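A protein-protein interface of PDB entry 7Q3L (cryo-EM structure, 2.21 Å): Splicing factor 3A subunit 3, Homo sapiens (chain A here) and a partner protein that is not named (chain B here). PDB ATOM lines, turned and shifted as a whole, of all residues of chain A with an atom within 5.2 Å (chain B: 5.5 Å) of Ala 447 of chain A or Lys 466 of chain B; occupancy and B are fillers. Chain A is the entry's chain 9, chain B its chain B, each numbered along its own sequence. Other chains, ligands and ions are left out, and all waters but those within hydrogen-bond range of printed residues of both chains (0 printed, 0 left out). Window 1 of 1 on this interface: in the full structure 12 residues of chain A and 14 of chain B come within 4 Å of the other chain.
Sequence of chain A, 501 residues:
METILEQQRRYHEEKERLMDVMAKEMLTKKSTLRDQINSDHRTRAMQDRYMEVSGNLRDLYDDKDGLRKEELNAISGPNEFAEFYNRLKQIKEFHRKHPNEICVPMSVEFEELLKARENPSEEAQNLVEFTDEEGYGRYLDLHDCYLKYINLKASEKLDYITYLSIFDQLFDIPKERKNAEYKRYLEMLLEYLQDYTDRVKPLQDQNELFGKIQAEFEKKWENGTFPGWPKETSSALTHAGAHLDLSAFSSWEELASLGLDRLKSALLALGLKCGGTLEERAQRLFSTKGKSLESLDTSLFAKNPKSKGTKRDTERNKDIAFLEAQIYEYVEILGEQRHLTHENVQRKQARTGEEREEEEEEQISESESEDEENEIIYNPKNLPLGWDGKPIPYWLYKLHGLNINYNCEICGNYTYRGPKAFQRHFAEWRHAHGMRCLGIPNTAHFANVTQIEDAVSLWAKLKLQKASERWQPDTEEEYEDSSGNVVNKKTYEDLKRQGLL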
ATOM      1  N   PHE A 426     -17.748   8.071  -7.918  1.00  0.00           N
ATOM      2  CA  PHE A 426     -17.004   9.321  -8.079  1.00  0.00           C
ATOM      3  C   PHE A 426     -15.616   9.283  -7.415  1.00  0.00           C
ATOM      4  O   PHE A 426     -14.777  10.135  -7.698  1.00  0.00           O
ATOM      5  CB  PHE A 426     -17.866  10.519  -7.656  1.00  0.00           C
ATOM      6  CG  PHE A 426     -19.201  10.536  -8.368  1.00  0.00           C
ATOM      7  CD1 PHE A 426     -19.306  11.003  -9.675  1.00  0.00           C
ATOM      8  CD2 PHE A 426     -20.345  10.023  -7.763  1.00  0.00           C
ATOM      9  CE1 PHE A 426     -20.511  10.926 -10.367  1.00  0.00           C
ATOM     10  CE2 PHE A 426     -21.551   9.945  -8.452  1.00  0.00           C
ATOM     11  CZ  PHE A 426     -21.628  10.384  -9.758  1.00  0.00           C
ATOM     12  N   ASN A 442     -10.548  15.237 -10.214  1.00  0.00           N
ATOM     13  CA  ASN A 442     -11.792  14.704  -9.672  1.00  0.00           C
ATOM     14  C   ASN A 442     -12.080  15.334  -8.307  1.00  0.00           C
ATOM     15  O   ASN A 442     -12.088  14.627  -7.297  1.00  0.00           O
ATOM     16  CB  ASN A 442     -11.771  13.171  -9.594  1.00  0.00           C
ATOM     17  CG  ASN A 442     -13.130  12.523  -9.767  1.00  0.00           C
ATOM     18  OD1 ASN A 442     -13.205  11.312  -9.975  1.00  0.00           O
ATOM     19  ND2 ASN A 442     -14.197  13.312  -9.713  1.00  0.00           N
ATOM     20  N   THR A 443     -12.350  16.653  -8.280  1.00  0.00           N
ATOM     21  CA  THR A 443     -12.644  17.366  -7.036  1.00  0.00           C
ATOM     22  C   THR A 443     -14.097  17.116  -6.622  1.00  0.00           C
ATOM     23  O   THR A 443     -14.888  16.691  -7.456  1.00  0.00           O
ATOM     24  CB  THR A 443     -12.335  18.866  -7.154  1.00  0.00           C
ATOM     25  OG1 THR A 443     -13.205  19.436  -8.131  1.00  0.00           O
ATOM     26  CG2 THR A 443     -10.897  19.151  -7.532  1.00  0.00           C
ATOM     27  N   ALA A 444     -14.432  17.375  -5.345  1.00  0.00           N
ATOM     28  CA  ALA A 444     -15.791  17.244  -4.833  1.00  0.00           C
ATOM     29  C   ALA A 444     -16.796  17.974  -5.728  1.00  0.00           C
ATOM     30  O   ALA A 444     -17.961  17.581  -5.802  1.00  0.00           O
ATOM     31  CB  ALA A 444     -15.853  17.734  -3.407  1.00  0.00           C
ATOM     32  N   HIS A 445     -16.324  19.028  -6.414  1.00  0.00           N
ATOM     33  CA  HIS A 445     -17.139  19.786  -7.356  1.00  0.00           C
ATOM     34  C   HIS A 445     -17.759  18.874  -8.425  1.00  0.00           C
ATOM     35  O   HIS A 445     -18.890  19.114  -8.837  1.00  0.00           O
ATOM     36  CB  HIS A 445     -16.276  20.880  -8.005  1.00  0.00           C
ATOM     37  CG  HIS A 445     -15.681  21.798  -6.998  1.00  0.00           C
ATOM     38  ND1 HIS A 445     -14.475  21.555  -6.378  1.00  0.00           N
ATOM     39  CD2 HIS A 445     -16.171  22.921  -6.442  1.00  0.00           C
ATOM     40  CE1 HIS A 445     -14.266  22.495  -5.480  1.00  0.00           C
ATOM     41  NE2 HIS A 445     -15.286  23.348  -5.501  1.00  0.00           N
ATOM     42  N   PHE A 446     -17.046  17.808  -8.828  1.00  0.00           N
ATOM     43  CA  PHE A 446     -17.473  16.864  -9.854  1.00  0.00           C
ATOM     44  C   PHE A 446     -18.116  15.591  -9.290  1.00  0.00           C
ATOM     45  O   PHE A 446     -18.582  14.746 -10.058  1.00  0.00           O
ATOM     46  CB  PHE A 446     -16.291  16.524 -10.762  1.00  0.00           C
ATOM     47  CG  PHE A 446     -15.647  17.743 -11.378  1.00  0.00           C
ATOM     48  CD1 PHE A 446     -16.193  18.338 -12.508  1.00  0.00           C
ATOM     49  CD2 PHE A 446     -14.510  18.312 -10.817  1.00  0.00           C
ATOM     50  CE1 PHE A 446     -15.621  19.470 -13.083  1.00  0.00           C
ATOM     51  CE2 PHE A 446     -13.942  19.449 -11.384  1.00  0.00           C
ATOM     52  CZ  PHE A 446     -14.492  20.019 -12.516  1.00  0.00           C
ATOM     53  N   ALA A 447     -18.177  15.428  -7.962  1.00  0.00           N
ATOM     54  CA  ALA A 447     -19.016  14.380  -7.386  1.00  0.00           C
ATOM     55  C   ALA A 447     -20.468  14.588  -7.828  1.00  0.00           C
ATOM     56  O   ALA A 447     -20.933  15.720  -7.891  1.00  0.00           O
ATOM     57  CB  ALA A 447     -18.884  14.371  -5.881  1.00  0.00           C
ATOM     58  N   ASN A 448     -21.173  13.491  -8.132  1.00  0.00           N
ATOM     59  CA  ASN A 448     -22.514  13.454  -8.712  1.00  0.00           C
ATOM     60  C   ASN A 448     -22.620  13.950 -10.172  1.00  0.00           C
ATOM     61  O   ASN A 448     -23.724  13.892 -10.727  1.00  0.00           O
ATOM     62  CB  ASN A 448     -23.540  14.116  -7.772  1.00  0.00           C
ATOM     63  CG  ASN A 448     -23.478  13.624  -6.337  1.00  0.00           C
ATOM     64  OD1 ASN A 448     -23.371  12.431  -6.084  1.00  0.00           O
ATOM     65  ND2 ASN A 448     -23.584  14.521  -5.376  1.00  0.00           N
ATOM     66  N   VAL A 449     -21.494  14.165 -10.887  1.00  0.00           N
ATOM     67  CA  VAL A 449     -21.498  14.493 -12.315  1.00  0.00           C
ATOM     68  C   VAL A 449     -21.107  13.282 -13.175  1.00  0.00           C
ATOM     69  O   VAL A 449     -19.969  12.811 -13.136  1.00  0.00           O
ATOM     70  CB  VAL A 449     -20.609  15.718 -12.610  1.00  0.00           C
ATOM     71  CG1 VAL A 449     -20.384  15.962 -14.099  1.00  0.00           C
ATOM     72  CG2 VAL A 449     -21.164  16.966 -11.949  1.00  0.00           C
ATOM     73  N   LEU A 458     -18.574  22.454 -16.728  1.00  0.00           N
ATOM     74  CA  LEU A 458     -18.323  22.727 -15.319  1.00  0.00           C
ATOM     75  C   LEU A 458     -16.826  22.937 -15.049  1.00  0.00           C
ATOM     76  O   LEU A 458     -16.481  23.858 -14.317  1.00  0.00           O
ATOM     77  CB  LEU A 458     -18.940  21.595 -14.487  1.00  0.00           C
ATOM     78  CG  LEU A 458     -18.752  21.647 -12.969  1.00  0.00           C
ATOM     79  CD1 LEU A 458     -19.388  22.889 -12.349  1.00  0.00           C
ATOM     80  CD2 LEU A 458     -19.349  20.403 -12.331  1.00  0.00           C
ATOM     81  N   LYS A 461     -16.119  26.518 -16.313  1.00  0.00           N
ATOM     82  CA  LYS A 461     -16.609  27.517 -15.361  1.00  0.00           C
ATOM     83  C   LYS A 461     -15.785  27.535 -14.065  1.00  0.00           C
ATOM     84  O   LYS A 461     -15.421  28.609 -13.590  1.00  0.00           O
ATOM     85  CB  LYS A 461     -18.139  27.458 -15.215  1.00  0.00           C
ATOM     86  CG  LYS A 461     -18.737  26.917 -13.917  1.00  0.00           C
ATOM     87  CD  LYS A 461     -18.805  27.906 -12.760  1.00  0.00           C
ATOM     88  CE  LYS A 461     -19.541  27.349 -11.558  1.00  0.00           C
ATOM     89  NZ  LYS A 461     -19.598  28.337 -10.452  1.00  0.00           N
ATOM     90  N   THR B 461     -31.580  19.810 -13.776  1.00  0.00           N
ATOM     91  CA  THR B 461     -30.644  18.690 -13.705  1.00  0.00           C
ATOM     92  C   THR B 461     -29.511  19.004 -12.719  1.00  0.00           C
ATOM     93  O   THR B 461     -29.228  20.171 -12.462  1.00  0.00           O
ATOM     94  CB  THR B 461     -30.184  18.236 -15.101  1.00  0.00           C
ATOM     95  OG1 THR B 461     -29.195  17.216 -14.956  1.00  0.00           O
ATOM     96  CG2 THR B 461     -29.585  19.334 -15.953  1.00  0.00           C
ATOM     97  N   VAL B 462     -28.822  17.974 -12.191  1.00  0.00           N
ATOM     98  CA  VAL B 462     -27.679  18.168 -11.298  1.00  0.00           C
ATOM     99  C   VAL B 462     -26.577  19.006 -11.953  1.00  0.00           C
ATOM    100  O   VAL B 462     -25.996  19.868 -11.299  1.00  0.00           O
ATOM    101  CB  VAL B 462     -27.124  16.869 -10.679  1.00  0.00           C
ATOM    102  CG1 VAL B 462     -28.133  16.204  -9.767  1.00  0.00           C
ATOM    103  CG2 VAL B 462     -26.541  15.880 -11.684  1.00  0.00           C
ATOM    104  N   ALA B 463     -26.350  18.800 -13.261  1.00  0.00           N
ATOM    105  CA  ALA B 463     -25.428  19.553 -14.110  1.00  0.00           C
ATOM    106  C   ALA B 463     -25.693  21.064 -14.061  1.00  0.00           C
ATOM    107  O   ALA B 463     -24.818  21.896 -13.804  1.00  0.00           O
ATOM    108  CB  ALA B 463     -25.587  19.036 -15.522  1.00  0.00           C
ATOM    109  N   GLU B 464     -26.957  21.412 -14.293  1.00  0.00           N
ATOM    110  CA  GLU B 464     -27.474  22.770 -14.365  1.00  0.00           C
ATOM    111  C   GLU B 464     -27.346  23.469 -13.009  1.00  0.00           C
ATOM    112  O   GLU B 464     -26.791  24.563 -12.940  1.00  0.00           O
ATOM    113  CB  GLU B 464     -28.898  22.632 -14.896  1.00  0.00           C
ATOM    114  CG  GLU B 464     -29.796  23.853 -14.886  1.00  0.00           C
ATOM    115  CD  GLU B 464     -31.186  23.503 -15.403  1.00  0.00           C
ATOM    116  OE1 GLU B 464     -31.555  22.294 -15.352  1.00  0.00           O
ATOM    117  OE2 GLU B 464     -31.907  24.426 -15.838  1.00  0.00           O
ATOM    118  N   LEU B 465     -27.770  22.804 -11.926  1.00  0.00           N
ATOM    119  CA  LEU B 465     -27.600  23.318 -10.572  1.00  0.00           C
ATOM    120  C   LEU B 465     -26.119  23.466 -10.196  1.00  0.00           C
ATOM    121  O   LEU B 465     -25.749  24.475  -9.606  1.00  0.00           O
ATOM    122  CB  LEU B 465     -28.380  22.437  -9.591  1.00  0.00           C
ATOM    123  CG  LEU B 465     -28.406  22.897  -8.130  1.00  0.00           C
ATOM    124  CD1 LEU B 465     -28.995  24.297  -7.967  1.00  0.00           C
ATOM    125  CD2 LEU B 465     -29.189  21.913  -7.277  1.00  0.00           C
ATOM    126  N   LYS B 466     -25.264  22.502 -10.566  1.00  0.00           N
ATOM    127  CA  LYS B 466     -23.819  22.568 -10.348  1.00  0.00           C
ATOM    128  C   LYS B 466     -23.190  23.801 -11.006  1.00  0.00           C
ATOM    129  O   LYS B 466     -22.321  24.425 -10.413  1.00  0.00           O
ATOM    130  CB  LYS B 466     -23.124  21.306 -10.874  1.00  0.00           C
ATOM    131  CG  LYS B 466     -23.256  20.059 -10.009  1.00  0.00           C
ATOM    132  CD  LYS B 466     -22.169  19.942  -8.962  1.00  0.00           C
ATOM    133  CE  LYS B 466     -22.261  18.636  -8.206  1.00  0.00           C
ATOM    134  NZ  LYS B 466     -21.133  18.473  -7.258  1.00  0.00           N
ATOM    135  N   GLN B 467     -23.615  24.158 -12.222  1.00  0.00           N
ATOM    136  CA  GLN B 467     -23.022  25.282 -12.940  1.00  0.00           C
ATOM    137  C   GLN B 467     -23.575  26.646 -12.497  1.00  0.00           C
ATOM    138  O   GLN B 467     -22.827  27.617 -12.495  1.00  0.00           O
ATOM    139  CB  GLN B 467     -23.052  25.024 -14.447  1.00  0.00           C
ATOM    140  CG  GLN B 467     -22.190  23.828 -14.833  1.00  0.00           C
ATOM    141  CD  GLN B 467     -21.894  23.701 -16.308  1.00  0.00           C
ATOM    142  OE1 GLN B 467     -21.531  24.665 -16.977  1.00  0.00           O
ATOM    143  NE2 GLN B 467     -21.987  22.491 -16.840  1.00  0.00           N
ATOM    144  N   LEU B 468     -24.857  26.729 -12.100  1.00  0.00           N
ATOM    145  CA  LEU B 468     -25.519  27.964 -11.675  1.00  0.00           C
ATOM    146  C   LEU B 468     -25.003  28.563 -10.355  1.00  0.00           C
ATOM    147  O   LEU B 468     -25.370  29.693 -10.024  1.00  0.00           O
ATOM    148  CB  LEU B 468     -27.028  27.713 -11.566  1.00  0.00           C
ATOM    149  CG  LEU B 468     -27.830  27.649 -12.866  1.00  0.00           C
ATOM    150  CD1 LEU B 468     -29.233  27.121 -12.596  1.00  0.00           C
ATOM    151  CD2 LEU B 468     -27.897  29.010 -13.545  1.00  0.00           C
ATOM    152  N   VAL B 469     -24.174  27.837  -9.581  1.00  0.00           N
ATOM    153  CA  VAL B 469     -23.900  28.196  -8.186  1.00  0.00           C
ATOM    154  C   VAL B 469     -22.421  28.486  -7.903  1.00  0.00           C
ATOM    155  O   VAL B 469     -21.515  27.929  -8.522  1.00  0.00           O
ATOM    156  CB  VAL B 469     -24.462  27.157  -7.192  1.00  0.00           C
ATOM    157  CG1 VAL B 469     -25.965  27.001  -7.358  1.00  0.00           C
ATOM    158  CG2 VAL B 469     -23.760  25.807  -7.312  1.00  0.00           C
ATOM    159  N   PRO B 472     -20.143  24.588  -6.292  1.00  0.00           N
ATOM    160  CA  PRO B 472     -20.622  23.298  -6.798  1.00  0.00           C
ATOM    161  C   PRO B 472     -20.305  22.074  -5.937  1.00  0.00           C
ATOM    162  O   PRO B 472     -20.960  21.053  -6.078  1.00  0.00           O
ATOM    163  CB  PRO B 472     -19.977  23.183  -8.189  1.00  0.00           C
ATOM    164  CG  PRO B 472     -19.650  24.619  -8.569  1.00  0.00           C
ATOM    165  CD  PRO B 472     -19.267  25.271  -7.256  1.00  0.00           C
ATOM    166  N   ASP B 473     -19.327  22.197  -5.031  1.00  0.00           N
ATOM    167  CA  ASP B 473     -18.925  21.127  -4.127  1.00  0.00           C
ATOM    168  C   ASP B 473     -19.928  20.847  -3.000  1.00  0.00           C
ATOM    169  O   ASP B 473     -19.822  19.792  -2.374  1.00  0.00           O
ATOM    170  CB  ASP B 473     -17.506  21.338  -3.583  1.00  0.00           C
ATOM    171  CG  ASP B 473     -17.160  22.712  -3.014  1.00  0.00           C
ATOM    172  OD1 ASP B 473     -16.307  22.763  -2.115  1.00  0.00           O
ATOM    173  OD2 ASP B 473     -17.687  23.749  -3.501  1.00  0.00           O
ATOM    174  N   VAL B 475     -23.253  20.684  -3.717  1.00  0.00           N
ATOM    175  CA  VAL B 475     -24.420  20.169  -4.431  1.00  0.00           C
ATOM    176  C   VAL B 475     -24.445  18.637  -4.421  1.00  0.00           C
ATOM    177  O   VAL B 475     -23.636  17.972  -5.074  1.00  0.00           O
ATOM    178  CB  VAL B 475     -24.542  20.737  -5.862  1.00  0.00           C
ATOM    179  CG1 VAL B 475     -25.784  20.243  -6.587  1.00  0.00           C
ATOM    180  CG2 VAL B 475     -24.515  22.252  -5.883  1.00  0.00           C
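Lys 466 of chain B touches just these residues of chain A: Ala 444, His 445, Ala 447 and Leu 458.
Of the printed residues of chain B, Leu 458 of chain A touches Lys 466 and Gln 467.
Of the printed residues of chain A, Asp 473 of chain B touches Ala 444 (3.97 Å) and His 445 (3.2 Å).
Phe 446 of chain A touches none of the printed residues of chain B.
The nearest printed residue of chain A that does not touch Lys 466 of chain B is Lys 461 of chain A (4.2 Å).
The side-chain hydroxyl (OG1) of Thr 443 of chain A lies within hydrogen-bond range of a ring nitrogen (ND1) of His 445 of chain A (3.0 Å).
The backbone carbonyl oxygen of Pro 472 of chain B sits at hydrogen-bond distance from the side-chain amino group of Lys 466 of chain B (2.8 Å).
The side-chain amino group of Lys 466 of chain B lies within hydrogen-bond range of the backbone carbonyl oxygen of Val 475 of chain B (3.4 Å).
NE2 of His 445 of chain A sits at hydrogen-bond distance from OD2 of Asp 473 of chain B (3.2 Å).
The backbone carbonyl oxygen (O) of Val 475 of chain B is in hydrogen-bond range of the side-chain amide nitrogen (ND2) of Asn 448 of chain A (3.5 Å).
The backbone carbonyl oxygen of Val 469 of chain B lies within hydrogen-bond range of the side-chain amino group of Lys 461 of chain A.
O of Ala 447 of chain A is in hydrogen-bond range of NZ of Lys 466 of chain B (2.8 Å).
The side-chain amide nitrogen of Gln 467 of chain B lies close to the backbone NH of Leu 458 of chain A (3.4 Å).
The side-chain amino group (NZ) of Lys 466 of chain B is in hydrogen-bond range of the backbone carbonyl oxygen (O) of His 445 of chain A, at 2.8 Å.
Of the 11 printed residues of chain A, 6 touch a printed residue of chain B.
Hydrophobic or aromatic side chains of chain A that line the printed part of chain B: Ala 444, His 445 and Leu 458.
Along chain A the printed residues that touch a printed residue of chain B span positions 444 to 461.
Printed residues of chain B that touch a printed residue of chain A: Val 462, Lys 466, Gln 467, Val 469, Pro 472, Asp 473 and Val 475.
Hydrophobic or aromatic side chains of chain B that line the printed part of chain A: Val 462 and Pro 472.
Among the printed residues, no Asp or Glu carboxylate lies within 4 Å of a Lys or Arg side-chain nitrogen of the other chain.
Among the printed residues, pairs that only touch across the chains: Ala 444 of chain A with Lys 466 of chain B, Ala 444 of chain A with Asp 473 of chain B, His 445 of chain A with Pro 472 of chain B, Asn 448 of chain A with Val 462 of chain B, Leu 458 of chain A with Lys 466 of chain B and Lys 461 of chain A with Gln 467 of chain B.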
